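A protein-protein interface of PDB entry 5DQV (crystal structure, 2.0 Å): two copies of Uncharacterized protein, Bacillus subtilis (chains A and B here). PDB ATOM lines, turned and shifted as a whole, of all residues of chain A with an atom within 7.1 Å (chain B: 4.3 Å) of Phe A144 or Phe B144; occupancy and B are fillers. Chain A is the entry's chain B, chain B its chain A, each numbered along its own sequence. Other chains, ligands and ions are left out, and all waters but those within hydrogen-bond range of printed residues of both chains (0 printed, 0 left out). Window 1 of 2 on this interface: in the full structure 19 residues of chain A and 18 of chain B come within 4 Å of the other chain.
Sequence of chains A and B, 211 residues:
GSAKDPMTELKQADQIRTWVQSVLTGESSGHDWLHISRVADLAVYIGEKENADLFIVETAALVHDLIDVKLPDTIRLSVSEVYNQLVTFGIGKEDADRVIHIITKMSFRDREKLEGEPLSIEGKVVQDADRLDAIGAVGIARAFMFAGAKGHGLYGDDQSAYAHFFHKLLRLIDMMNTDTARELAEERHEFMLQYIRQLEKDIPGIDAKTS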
ATOM      1  N   ALA A 137     -15.760   8.435  -3.263  1.00  0.00           N
ATOM      2  CA  ALA A 137     -14.954   8.812  -2.135  1.00  0.00           C
ATOM      3  C   ALA A 137     -15.766   8.747  -0.865  1.00  0.00           C
ATOM      4  O   ALA A 137     -15.261   8.279   0.173  1.00  0.00           O
ATOM      5  CB  ALA A 137     -14.365  10.240  -2.366  1.00  0.00           C
ATOM      6  N   VAL A 138     -17.033   9.147  -0.913  1.00  0.00           N
ATOM      7  CA  VAL A 138     -17.865   9.087   0.291  1.00  0.00           C
ATOM      8  C   VAL A 138     -18.154   7.619   0.642  1.00  0.00           C
ATOM      9  O   VAL A 138     -18.048   7.209   1.812  1.00  0.00           O
ATOM     10  CB  VAL A 138     -19.169   9.924   0.174  1.00  0.00           C
ATOM     11  CG1 VAL A 138     -20.083   9.377  -0.905  1.00  0.00           C
ATOM     12  CG2 VAL A 138     -19.897   9.940   1.522  1.00  0.00           C
ATOM     13  N   GLY A 139     -18.513   6.814  -0.365  1.00  0.00           N
ATOM     14  CA  GLY A 139     -18.729   5.383  -0.152  1.00  0.00           C
ATOM     15  C   GLY A 139     -17.527   4.659   0.483  1.00  0.00           C
ATOM     16  O   GLY A 139     -17.687   3.825   1.386  1.00  0.00           O
ATOM     17  N   ILE A 140     -16.315   4.994   0.034  1.00  0.00           N
ATOM     18  CA  ILE A 140     -15.080   4.395   0.570  1.00  0.00           C
ATOM     19  C   ILE A 140     -14.931   4.765   2.061  1.00  0.00           C
ATOM     20  O   ILE A 140     -14.692   3.923   2.919  1.00  0.00           O
ATOM     21  CB  ILE A 140     -13.888   4.894  -0.211  1.00  0.00           C
ATOM     22  CG1 ILE A 140     -13.824   4.271  -1.590  1.00  0.00           C
ATOM     23  CG2 ILE A 140     -12.558   4.693   0.591  1.00  0.00           C
ATOM     24  CD1 ILE A 140     -13.042   5.191  -2.611  1.00  0.00           C
ATOM     25  N   ALA A 141     -15.112   6.038   2.365  1.00  0.00           N
ATOM     26  CA  ALA A 141     -15.063   6.496   3.752  1.00  0.00           C
ATOM     27  C   ALA A 141     -16.028   5.708   4.635  1.00  0.00           C
ATOM     28  O   ALA A 141     -15.649   5.209   5.687  1.00  0.00           O
ATOM     29  CB  ALA A 141     -15.358   7.987   3.836  1.00  0.00           C
ATOM     30  N   ARG A 142     -17.266   5.571   4.164  1.00  0.00           N
ATOM     31  CA  ARG A 142     -18.305   4.915   4.928  1.00  0.00           C
ATOM     32  C   ARG A 142     -17.963   3.455   5.141  1.00  0.00           C
ATOM     33  O   ARG A 142     -18.204   2.916   6.219  1.00  0.00           O
ATOM     34  CB  ARG A 142     -19.682   5.085   4.244  1.00  0.00           C
ATOM     35  CG  ARG A 142     -20.226   6.487   4.297  1.00  0.00           C
ATOM     36  CD  ARG A 142     -21.594   6.619   3.571  1.00  0.00           C
ATOM     37  NE  ARG A 142     -22.642   5.955   4.328  1.00  0.00           N
ATOM     38  CZ  ARG A 142     -23.673   5.287   3.826  1.00  0.00           C
ATOM     39  NH1 ARG A 142     -23.881   5.191   2.499  1.00  0.00           N
ATOM     40  NH2 ARG A 142     -24.506   4.696   4.682  1.00  0.00           N
ATOM     41  N   ALA A 143     -17.342   2.828   4.133  1.00  0.00           N
ATOM     42  CA  ALA A 143     -17.017   1.403   4.180  1.00  0.00           C
ATOM     43  C   ALA A 143     -15.975   1.180   5.260  1.00  0.00           C
ATOM     44  O   ALA A 143     -16.064   0.241   6.055  1.00  0.00           O
ATOM     45  CB  ALA A 143     -16.471   0.943   2.827  1.00  0.00           C
ATOM     46  N   PHE A 144     -14.978   2.061   5.298  1.00  0.00           N
ATOM     47  CA  PHE A 144     -13.957   1.935   6.306  1.00  0.00           C
ATOM     48  C   PHE A 144     -14.488   2.321   7.679  1.00  0.00           C
ATOM     49  O   PHE A 144     -14.158   1.685   8.649  1.00  0.00           O
ATOM     50  CB  PHE A 144     -12.693   2.686   5.905  1.00  0.00           C
ATOM     51  CG  PHE A 144     -11.907   1.972   4.827  1.00  0.00           C
ATOM     52  CD1 PHE A 144     -11.366   0.723   5.071  1.00  0.00           C
ATOM     53  CD2 PHE A 144     -11.734   2.550   3.571  1.00  0.00           C
ATOM     54  CE1 PHE A 144     -10.650   0.070   4.104  1.00  0.00           C
ATOM     55  CE2 PHE A 144     -11.040   1.884   2.586  1.00  0.00           C
ATOM     56  CZ  PHE A 144     -10.505   0.655   2.850  1.00  0.00           C
ATOM     57  N   MET A 145     -15.337   3.342   7.752  1.00  0.00           N
ATOM     58  CA  MET A 145     -15.982   3.709   9.012  1.00  0.00           C
ATOM     59  C   MET A 145     -16.774   2.539   9.592  1.00  0.00           C
ATOM     60  O   MET A 145     -16.685   2.236  10.781  1.00  0.00           O
ATOM     61  CB  MET A 145     -16.846   4.981   8.835  1.00  0.00           C
ATOM     62  CG  MET A 145     -17.941   5.227   9.895  1.00  0.00           C
ATOM     63  SD  MET A 145     -19.080   6.612   9.521  1.00  0.00           S
ATOM     64  CE  MET A 145     -17.772   7.850   9.183  1.00  0.00           C
ATOM     65  N   PHE A 146     -17.558   1.886   8.762  1.00  0.00           N
ATOM     66  CA  PHE A 146     -18.397   0.772   9.218  1.00  0.00           C
ATOM     67  C   PHE A 146     -17.521  -0.340   9.815  1.00  0.00           C
ATOM     68  O   PHE A 146     -17.823  -0.940  10.858  1.00  0.00           O
ATOM     69  CB  PHE A 146     -19.205   0.231   8.028  1.00  0.00           C
ATOM     70  CG  PHE A 146     -20.180  -0.873   8.391  1.00  0.00           C
ATOM     71  CD1 PHE A 146     -21.388  -0.569   8.997  1.00  0.00           C
ATOM     72  CD2 PHE A 146     -19.888  -2.199   8.125  1.00  0.00           C
ATOM     73  CE1 PHE A 146     -22.314  -1.587   9.329  1.00  0.00           C
ATOM     74  CE2 PHE A 146     -20.813  -3.238   8.458  1.00  0.00           C
ATOM     75  CZ  PHE A 146     -22.004  -2.930   9.064  1.00  0.00           C
ATOM     76  N   ALA A 147     -16.419  -0.595   9.137  1.00  0.00           N
ATOM     77  CA  ALA A 147     -15.507  -1.667   9.504  1.00  0.00           C
ATOM     78  C   ALA A 147     -14.862  -1.355  10.831  1.00  0.00           C
ATOM     79  O   ALA A 147     -14.656  -2.225  11.679  1.00  0.00           O
ATOM     80  CB  ALA A 147     -14.462  -1.810   8.437  1.00  0.00           C
ATOM     81  N   GLY A 148     -14.536  -0.105  11.025  1.00  0.00           N
ATOM     82  CA  GLY A 148     -13.995   0.326  12.301  1.00  0.00           C
ATOM     83  C   GLY A 148     -14.991   0.193  13.437  1.00  0.00           C
ATOM     84  O   GLY A 148     -14.648  -0.279  14.528  1.00  0.00           O
ATOM     85  N   ALA A 149     -16.209   0.644  13.187  1.00  0.00           N
ATOM     86  CA  ALA A 149     -17.296   0.544  14.174  1.00  0.00           C
ATOM     87  C   ALA A 149     -17.552  -0.905  14.591  1.00  0.00           C
ATOM     88  O   ALA A 149     -17.753  -1.190  15.776  1.00  0.00           O
ATOM     89  CB  ALA A 149     -18.573   1.172  13.635  1.00  0.00           C
ATOM     90  N   LYS A 150     -17.541  -1.815  13.626  1.00  0.00           N
ATOM     91  CA  LYS A 150     -17.905  -3.196  13.893  1.00  0.00           C
ATOM     92  C   LYS A 150     -16.711  -4.078  14.244  1.00  0.00           C
ATOM     93  O   LYS A 150     -16.870  -5.259  14.454  1.00  0.00           O
ATOM     94  CB  LYS A 150     -18.712  -3.775  12.731  1.00  0.00           C
ATOM     95  CG  LYS A 150     -20.009  -3.001  12.445  1.00  0.00           C
ATOM     96  CD  LYS A 150     -20.908  -2.830  13.690  1.00  0.00           C
ATOM     97  CE  LYS A 150     -22.065  -1.840  13.394  1.00  0.00           C
ATOM     98  NZ  LYS A 150     -22.985  -1.623  14.554  1.00  0.00           N
ATOM     99  N   HIS A 152     -14.156  -4.707  12.397  1.00  0.00           N
ATOM    100  CA  HIS A 152     -13.676  -5.436  11.233  1.00  0.00           C
ATOM    101  C   HIS A 152     -12.366  -4.845  10.702  1.00  0.00           C
ATOM    102  O   HIS A 152     -12.076  -3.664  10.892  1.00  0.00           O
ATOM    103  CB  HIS A 152     -14.696  -5.381  10.104  1.00  0.00           C
ATOM    104  CG  HIS A 152     -15.995  -6.040  10.413  1.00  0.00           C
ATOM    105  ND1 HIS A 152     -17.180  -5.629   9.844  1.00  0.00           N
ATOM    106  CD2 HIS A 152     -16.302  -7.082  11.216  1.00  0.00           C
ATOM    107  CE1 HIS A 152     -18.163  -6.401  10.274  1.00  0.00           C
ATOM    108  NE2 HIS A 152     -17.658  -7.280  11.119  1.00  0.00           N
ATOM    109  N   GLY A 153     -11.606  -5.690  10.011  1.00  0.00           N
ATOM    110  CA  GLY A 153     -10.312  -5.325   9.470  1.00  0.00           C
ATOM    111  C   GLY A 153     -10.367  -4.542   8.180  1.00  0.00           C
ATOM    112  O   GLY A 153     -11.382  -4.516   7.477  1.00  0.00           O
ATOM    113  N   LEU A 154      -9.250  -3.888   7.873  1.00  0.00           N
ATOM    114  CA  LEU A 154      -9.102  -3.153   6.628  1.00  0.00           C
ATOM    115  C   LEU A 154      -9.188  -4.131   5.432  1.00  0.00           C
ATOM    116  O   LEU A 154      -9.852  -3.844   4.418  1.00  0.00           O
ATOM    117  CB  LEU A 154      -7.750  -2.453   6.643  1.00  0.00           C
ATOM    118  CG  LEU A 154      -7.507  -1.239   5.790  1.00  0.00           C
ATOM    119  CD1 LEU A 154      -6.306  -0.441   6.423  1.00  0.00           C
ATOM    120  CD2 LEU A 154      -7.278  -1.612   4.303  1.00  0.00           C
ATOM    121  N   TYR A 155      -8.447  -5.230   5.580  1.00  0.00           N
ATOM    122  CA  TYR A 155      -8.374  -6.364   4.663  1.00  0.00           C
ATOM    123  C   TYR A 155      -8.011  -7.600   5.503  1.00  0.00           C
ATOM    124  O   TYR A 155      -7.865  -7.500   6.720  1.00  0.00           O
ATOM    125  CB  TYR A 155      -7.321  -6.171   3.563  1.00  0.00           C
ATOM    126  CG  TYR A 155      -5.934  -5.882   4.117  1.00  0.00           C
ATOM    127  CD1 TYR A 155      -5.601  -4.595   4.506  1.00  0.00           C
ATOM    128  CD2 TYR A 155      -4.978  -6.887   4.282  1.00  0.00           C
ATOM    129  CE1 TYR A 155      -4.365  -4.311   5.048  1.00  0.00           C
ATOM    130  CE2 TYR A 155      -3.715  -6.607   4.808  1.00  0.00           C
ATOM    131  CZ  TYR A 155      -3.436  -5.310   5.184  1.00  0.00           C
ATOM    132  OH  TYR A 155      -2.243  -4.956   5.708  1.00  0.00           O
ATOM    133  N   SER A 160     -14.066  -7.976   5.805  1.00  0.00           N
ATOM    134  CA  SER A 160     -13.296  -6.742   5.729  1.00  0.00           C
ATOM    135  C   SER A 160     -13.894  -5.725   4.769  1.00  0.00           C
ATOM    136  O   SER A 160     -14.727  -6.055   3.919  1.00  0.00           O
ATOM    137  CB  SER A 160     -11.864  -7.055   5.283  1.00  0.00           C
ATOM    138  OG  SER A 160     -11.848  -7.321   3.889  1.00  0.00           O
ATOM    139  N   ALA A 161     -13.427  -4.474   4.885  1.00  0.00           N
ATOM    140  CA  ALA A 161     -13.888  -3.412   4.018  1.00  0.00           C
ATOM    141  C   ALA A 161     -13.496  -3.685   2.575  1.00  0.00           C
ATOM    142  O   ALA A 161     -14.278  -3.448   1.645  1.00  0.00           O
ATOM    143  CB  ALA A 161     -13.328  -2.062   4.470  1.00  0.00           C
ATOM    144  N   TYR A 162     -12.268  -4.162   2.389  1.00  0.00           N
ATOM    145  CA  TYR A 162     -11.745  -4.414   1.054  1.00  0.00           C
ATOM    146  C   TYR A 162     -12.629  -5.420   0.334  1.00  0.00           C
ATOM    147  O   TYR A 162     -12.920  -5.271  -0.835  1.00  0.00           O
ATOM    148  CB  TYR A 162     -10.311  -4.913   1.146  1.00  0.00           C
ATOM    149  CG  TYR A 162      -9.668  -5.334  -0.167  1.00  0.00           C
ATOM    150  CD1 TYR A 162      -9.307  -4.393  -1.164  1.00  0.00           C
ATOM    151  CD2 TYR A 162      -9.362  -6.652  -0.386  1.00  0.00           C
ATOM    152  CE1 TYR A 162      -8.676  -4.834  -2.370  1.00  0.00           C
ATOM    153  CE2 TYR A 162      -8.754  -7.080  -1.557  1.00  0.00           C
ATOM    154  CZ  TYR A 162      -8.414  -6.182  -2.540  1.00  0.00           C
ATOM    155  OH  TYR A 162      -7.823  -6.720  -3.678  1.00  0.00           O
ATOM    156  N   PHE A 165     -15.981  -4.050  -1.102  1.00  0.00           N
ATOM    157  CA  PHE A 165     -15.928  -3.390  -2.428  1.00  0.00           C
ATOM    158  C   PHE A 165     -16.302  -4.319  -3.582  1.00  0.00           C
ATOM    159  O   PHE A 165     -17.033  -3.940  -4.503  1.00  0.00           O
ATOM    160  CB  PHE A 165     -14.548  -2.827  -2.748  1.00  0.00           C
ATOM    161  CG  PHE A 165     -14.125  -1.744  -1.860  1.00  0.00           C
ATOM    162  CD1 PHE A 165     -14.863  -0.590  -1.750  1.00  0.00           C
ATOM    163  CD2 PHE A 165     -12.945  -1.832  -1.176  1.00  0.00           C
ATOM    164  CE1 PHE A 165     -14.444   0.447  -0.925  1.00  0.00           C
ATOM    165  CE2 PHE A 165     -12.528  -0.791  -0.345  1.00  0.00           C
ATOM    166  CZ  PHE A 165     -13.292   0.331  -0.217  1.00  0.00           C
ATOM    167  N   TYR A 195      -8.961   4.247  -6.463  1.00  0.00           N
ATOM    168  CA  TYR A 195      -8.672   4.069  -5.022  1.00  0.00           C
ATOM    169  C   TYR A 195      -8.203   2.637  -4.760  1.00  0.00           C
ATOM    170  O   TYR A 195      -7.191   2.456  -4.122  1.00  0.00           O
ATOM    171  CB  TYR A 195      -9.843   4.425  -4.088  1.00  0.00           C
ATOM    172  CG  TYR A 195      -9.487   4.180  -2.637  1.00  0.00           C
ATOM    173  CD1 TYR A 195      -9.703   2.943  -2.058  1.00  0.00           C
ATOM    174  CD2 TYR A 195      -8.854   5.155  -1.869  1.00  0.00           C
ATOM    175  CE1 TYR A 195      -9.296   2.674  -0.750  1.00  0.00           C
ATOM    176  CE2 TYR A 195      -8.460   4.898  -0.547  1.00  0.00           C
ATOM    177  CZ  TYR A 195      -8.708   3.625   0.003  1.00  0.00           C
ATOM    178  OH  TYR A 195      -8.340   3.340   1.306  1.00  0.00           O
ATOM    179  N   LEU A 199      -4.668   1.344  -3.353  1.00  0.00           N
ATOM    180  CA  LEU A 199      -4.590   0.564  -2.122  1.00  0.00           C
ATOM    181  C   LEU A 199      -3.830  -0.749  -2.348  1.00  0.00           C
ATOM    182  O   LEU A 199      -2.958  -1.124  -1.563  1.00  0.00           O
ATOM    183  CB  LEU A 199      -5.989   0.263  -1.618  1.00  0.00           C
ATOM    184  CG  LEU A 199      -6.044  -0.261  -0.190  1.00  0.00           C
ATOM    185  CD1 LEU A 199      -5.499   0.796   0.920  1.00  0.00           C
ATOM    186  CD2 LEU A 199      -7.425  -0.742   0.083  1.00  0.00           C
ATOM    187  N   ILE A 206      -2.447  -7.643  -0.470  1.00  0.00           N
ATOM    188  CA  ILE A 206      -3.708  -7.328   0.204  1.00  0.00           C
ATOM    189  C   ILE A 206      -4.800  -8.395  -0.042  1.00  0.00           C
ATOM    190  O   ILE A 206      -5.688  -8.553   0.797  1.00  0.00           O
ATOM    191  CB  ILE A 206      -4.238  -5.953  -0.226  1.00  0.00           C
ATOM    192  CG1 ILE A 206      -5.469  -5.553   0.591  1.00  0.00           C
ATOM    193  CG2 ILE A 206      -4.532  -5.917  -1.729  1.00  0.00           C
ATOM    194  CD1 ILE A 206      -5.882  -4.100   0.375  1.00  0.00           C
ATOM    195  N   ILE B 140      -5.869   6.901   4.370  1.00  0.00           N
ATOM    196  CA  ILE B 140      -7.279   7.257   4.250  1.00  0.00           C
ATOM    197  C   ILE B 140      -8.128   6.215   4.932  1.00  0.00           C
ATOM    198  O   ILE B 140      -9.009   6.522   5.768  1.00  0.00           O
ATOM    199  CB  ILE B 140      -7.671   7.416   2.745  1.00  0.00           C
ATOM    200  CG1 ILE B 140      -7.115   8.734   2.181  1.00  0.00           C
ATOM    201  CG2 ILE B 140      -9.193   7.440   2.552  1.00  0.00           C
ATOM    202  CD1 ILE B 140      -6.969   8.690   0.687  1.00  0.00           C
ATOM    203  N   ALA B 141      -7.836   4.952   4.616  1.00  0.00           N
ATOM    204  CA  ALA B 141      -8.607   3.833   5.198  1.00  0.00           C
ATOM    205  C   ALA B 141      -8.473   3.833   6.696  1.00  0.00           C
ATOM    206  O   ALA B 141      -9.463   3.677   7.446  1.00  0.00           O
ATOM    207  CB  ALA B 141      -8.140   2.517   4.631  1.00  0.00           C
ATOM    208  N   ARG B 142      -7.254   4.074   7.150  1.00  0.00           N
ATOM    209  CA  ARG B 142      -7.010   4.020   8.583  1.00  0.00           C
ATOM    210  C   ARG B 142      -7.725   5.153   9.314  1.00  0.00           C
ATOM    211  O   ARG B 142      -8.263   4.944  10.399  1.00  0.00           O
ATOM    212  CB  ARG B 142      -5.516   4.008   8.867  1.00  0.00           C
ATOM    213  CG  ARG B 142      -4.845   2.719   8.507  1.00  0.00           C
ATOM    214  CD  ARG B 142      -3.355   2.807   8.790  1.00  0.00           C
ATOM    215  NE  ARG B 142      -3.148   2.771  10.234  1.00  0.00           N
ATOM    216  CZ  ARG B 142      -2.139   3.328  10.902  1.00  0.00           C
ATOM    217  NH1 ARG B 142      -1.160   4.000  10.291  1.00  0.00           N
ATOM    218  NH2 ARG B 142      -2.114   3.199  12.211  1.00  0.00           N
ATOM    219  N   ALA B 143      -7.760   6.327   8.700  1.00  0.00           N
ATOM    220  CA  ALA B 143      -8.407   7.502   9.325  1.00  0.00           C
ATOM    221  C   ALA B 143      -9.891   7.241   9.526  1.00  0.00           C
ATOM    222  O   ALA B 143     -10.457   7.527  10.588  1.00  0.00           O
ATOM    223  CB  ALA B 143      -8.218   8.734   8.472  1.00  0.00           C
ATOM    224  N   PHE B 144     -10.527   6.702   8.488  1.00  0.00           N
ATOM    225  CA  PHE B 144     -11.949   6.437   8.561  1.00  0.00           C
ATOM    226  C   PHE B 144     -12.264   5.265   9.489  1.00  0.00           C
ATOM    227  O   PHE B 144     -13.260   5.299  10.223  1.00  0.00           O
ATOM    228  CB  PHE B 144     -12.535   6.277   7.169  1.00  0.00           C
ATOM    229  CG  PHE B 144     -12.591   7.578   6.391  1.00  0.00           C
ATOM    230  CD1 PHE B 144     -13.335   8.658   6.871  1.00  0.00           C
ATOM    231  CD2 PHE B 144     -11.899   7.730   5.234  1.00  0.00           C
ATOM    232  CE1 PHE B 144     -13.341   9.887   6.192  1.00  0.00           C
ATOM    233  CE2 PHE B 144     -11.934   8.973   4.520  1.00  0.00           C
ATOM    234  CZ  PHE B 144     -12.660  10.011   4.993  1.00  0.00           C
ATOM    235  N   MET B 145     -11.419   4.232   9.489  1.00  0.00           N
ATOM    236  CA  MET B 145     -11.577   3.127  10.473  1.00  0.00           C
ATOM    237  C   MET B 145     -11.522   3.638  11.937  1.00  0.00           C
ATOM    238  O   MET B 145     -12.377   3.317  12.754  1.00  0.00           O
ATOM    239  CB  MET B 145     -10.484   2.086  10.246  1.00  0.00           C
ATOM    240  CG  MET B 145     -10.378   0.908  11.296  1.00  0.00           C
ATOM    241  SD  MET B 145      -8.836  -0.060  10.991  1.00  0.00           S
ATOM    242  CE  MET B 145      -8.772   0.090   9.160  1.00  0.00           C
ATOM    243  N   PHE B 146     -10.519   4.455  12.230  1.00  0.00           N
ATOM    244  CA  PHE B 146     -10.366   5.067  13.549  1.00  0.00           C
ATOM    245  C   PHE B 146     -11.598   5.867  13.947  1.00  0.00           C
ATOM    246  O   PHE B 146     -12.126   5.723  15.079  1.00  0.00           O
ATOM    247  CB  PHE B 146      -9.112   5.952  13.561  1.00  0.00           C
ATOM    248  CG  PHE B 146      -8.781   6.511  14.920  1.00  0.00           C
ATOM    249  CD1 PHE B 146      -7.983   5.787  15.811  1.00  0.00           C
ATOM    250  CD2 PHE B 146      -9.265   7.756  15.314  1.00  0.00           C
ATOM    251  CE1 PHE B 146      -7.674   6.301  17.079  1.00  0.00           C
ATOM    252  CE2 PHE B 146      -8.955   8.273  16.583  1.00  0.00           C
ATOM    253  CZ  PHE B 146      -8.164   7.546  17.458  1.00  0.00           C
ATOM    254  N   ALA B 147     -12.101   6.684  13.018  1.00  0.00           N
ATOM    255  CA  ALA B 147     -13.317   7.481  13.275  1.00  0.00           C
ATOM    256  C   ALA B 147     -14.510   6.599  13.633  1.00  0.00           C
ATOM    257  O   ALA B 147     -15.334   6.927  14.522  1.00  0.00           O
ATOM    258  CB  ALA B 147     -13.649   8.372  12.058  1.00  0.00           C
ATOM    259  N   GLY B 148     -14.643   5.504  12.884  1.00  0.00           N
ATOM    260  CA  GLY B 148     -15.721   4.541  13.114  1.00  0.00           C
ATOM    261  C   GLY B 148     -15.526   3.846  14.458  1.00  0.00           C
ATOM    262  O   GLY B 148     -16.487   3.603  15.184  1.00  0.00           O
ATOM    263  N   LEU B 154     -17.566  11.477   9.833  1.00  0.00           N
ATOM    264  CA  LEU B 154     -16.810  11.648   8.579  1.00  0.00           C
ATOM    265  C   LEU B 154     -16.210  13.051   8.431  1.00  0.00           C
ATOM    266  O   LEU B 154     -15.053  13.255   7.981  1.00  0.00           O
ATOM    267  CB  LEU B 154     -17.799  11.425   7.446  1.00  0.00           C
ATOM    268  CG  LEU B 154     -17.323  10.696   6.223  1.00  0.00           C
ATOM    269  CD1 LEU B 154     -18.553   9.917   5.568  1.00  0.00           C
ATOM    270  CD2 LEU B 154     -16.619  11.680   5.303  1.00  0.00           C
ATOM    271  N   ALA B 161     -12.855  12.656  10.883  1.00  0.00           N
ATOM    272  CA  ALA B 161     -11.767  12.164  10.073  1.00  0.00           C
ATOM    273  C   ALA B 161     -11.287  13.276   9.157  1.00  0.00           C
ATOM    274  O   ALA B 161     -10.075  13.490   8.995  1.00  0.00           O
ATOM    275  CB  ALA B 161     -12.230  10.926   9.238  1.00  0.00           C
ATOM    276  N   PHE B 165      -7.418  14.946   8.621  1.00  0.00           N
ATOM    277  CA  PHE B 165      -6.617  15.160   7.432  1.00  0.00           C
ATOM    278  C   PHE B 165      -5.921  16.521   7.466  1.00  0.00           C
ATOM    279  O   PHE B 165      -4.710  16.589   7.246  1.00  0.00           O
ATOM    280  CB  PHE B 165      -7.438  15.076   6.141  1.00  0.00           C
ATOM    281  CG  PHE B 165      -7.937  13.668   5.811  1.00  0.00           C
ATOM    282  CD1 PHE B 165      -7.066  12.649   5.615  1.00  0.00           C
ATOM    283  CD2 PHE B 165      -9.282  13.379   5.748  1.00  0.00           C
ATOM    284  CE1 PHE B 165      -7.550  11.319   5.356  1.00  0.00           C
ATOM    285  CE2 PHE B 165      -9.752  12.070   5.498  1.00  0.00           C
ATOM    286  CZ  PHE B 165      -8.897  11.067   5.303  1.00  0.00           C
ATOM    287  N   TYR B 195      -8.047  12.659  -3.017  1.00  0.00           N
ATOM    288  CA  TYR B 195      -9.173  12.076  -2.263  1.00  0.00           C
ATOM    289  C   TYR B 195     -10.011  13.199  -1.619  1.00  0.00           C
ATOM    290  O   TYR B 195     -11.235  13.250  -1.747  1.00  0.00           O
ATOM    291  CB  TYR B 195      -8.670  11.067  -1.215  1.00  0.00           C
ATOM    292  CG  TYR B 195      -9.829  10.456  -0.495  1.00  0.00           C
ATOM    293  CD1 TYR B 195     -10.377  11.110   0.592  1.00  0.00           C
ATOM    294  CD2 TYR B 195     -10.438   9.309  -0.947  1.00  0.00           C
ATOM    295  CE1 TYR B 195     -11.467  10.600   1.241  1.00  0.00           C
ATOM    296  CE2 TYR B 195     -11.555   8.800  -0.307  1.00  0.00           C
ATOM    297  CZ  TYR B 195     -12.055   9.493   0.798  1.00  0.00           C
ATOM    298  OH  TYR B 195     -13.166   9.081   1.500  1.00  0.00           O
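The side-chain hydroxyl (OH) of Tyr B195 is in hydrogen-bond range of the backbone carbonyl oxygen (O) of Ala A137, at 2.6 Å.
The backbone NH (N) of Tyr A162 sits at hydrogen-bond distance from the backbone carbonyl oxygen (O) of Leu A154 (3.2 Å).
Among the printed residues, pairs that only touch across the chains: Ala A149 with Gly B148 (3.3 Å), Met A145 with Phe B144 (3.4 Å), Ala A141 with Tyr B195 (3.4 Å), Met A145 with Gly B148 (3.4 Å), Gly A148 with Met B145 (3.4 Å), Tyr A195 with Ala B141 (3.4 Å), Phe A144 with Met B145 (3.5 Å), Phe A144 with Ala B141 (3.5 Å), Ala A141 with Phe B144 (3.6 Å), Met A145 with Leu B154 (3.7 Å), Leu A154 with Met B145 (3.7 Å), Phe A144 with Phe B144 (3.8 Å), Gly A148 with Gly B148 (3.8 Å) and Leu A154 with Ala B141 (3.9 Å).
Of the printed residues of chain B, Ala A137 touches Tyr B195 (2.6 Å). Of the printed residues of chain B, Ala A141 touches Phe B144 and Tyr B195. Phe A144 touches just these residues of chain B: Ala B141, Phe B144 and Met B145. Gly A153 touches none of the printed residues of chain B. Phe A165 touches none of the printed residues of chain B. Printed residues of chain A within 4 Å of Ala B141: Phe A144 (3.5 Å), Leu A154 (3.9 Å) and Tyr A195 (3.4 Å). Of the printed residues of chain A, Leu B154 touches Met A145. The nearest printed residue of chain B that does not touch Phe A144 is Ile B140 (5.3 Å). The nearest residue of chain A that does not touch Phe B144 is Ile A140 (5.3 Å). The nearest printed residue of chain B that does not touch Ala A141 is Leu B154 (4.1 Å).
Of the 25 printed residues of chain A, 8 touch a printed residue of chain B. Hydrophobic or aromatic side chains of chain A that line the printed part of chain B: Ala A137, Ala A141, Phe A144, Met A145, Ala A149, Leu A154 and Tyr A195. Among the printed residues, no Asp or Glu carboxylate lies within 4 Å of a Lys or Arg side-chain nitrogen of the other chain.
Ala A141 touches Phe B144, and with the chains exchanged Phe A144 touches Ala B141. Phe A144 touches its own counterpart, Phe B144. Met A145 touches Gly B148, and with the chains exchanged Gly A148 touches Met B145. Gly A148 touches its own counterpart, Gly B148.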
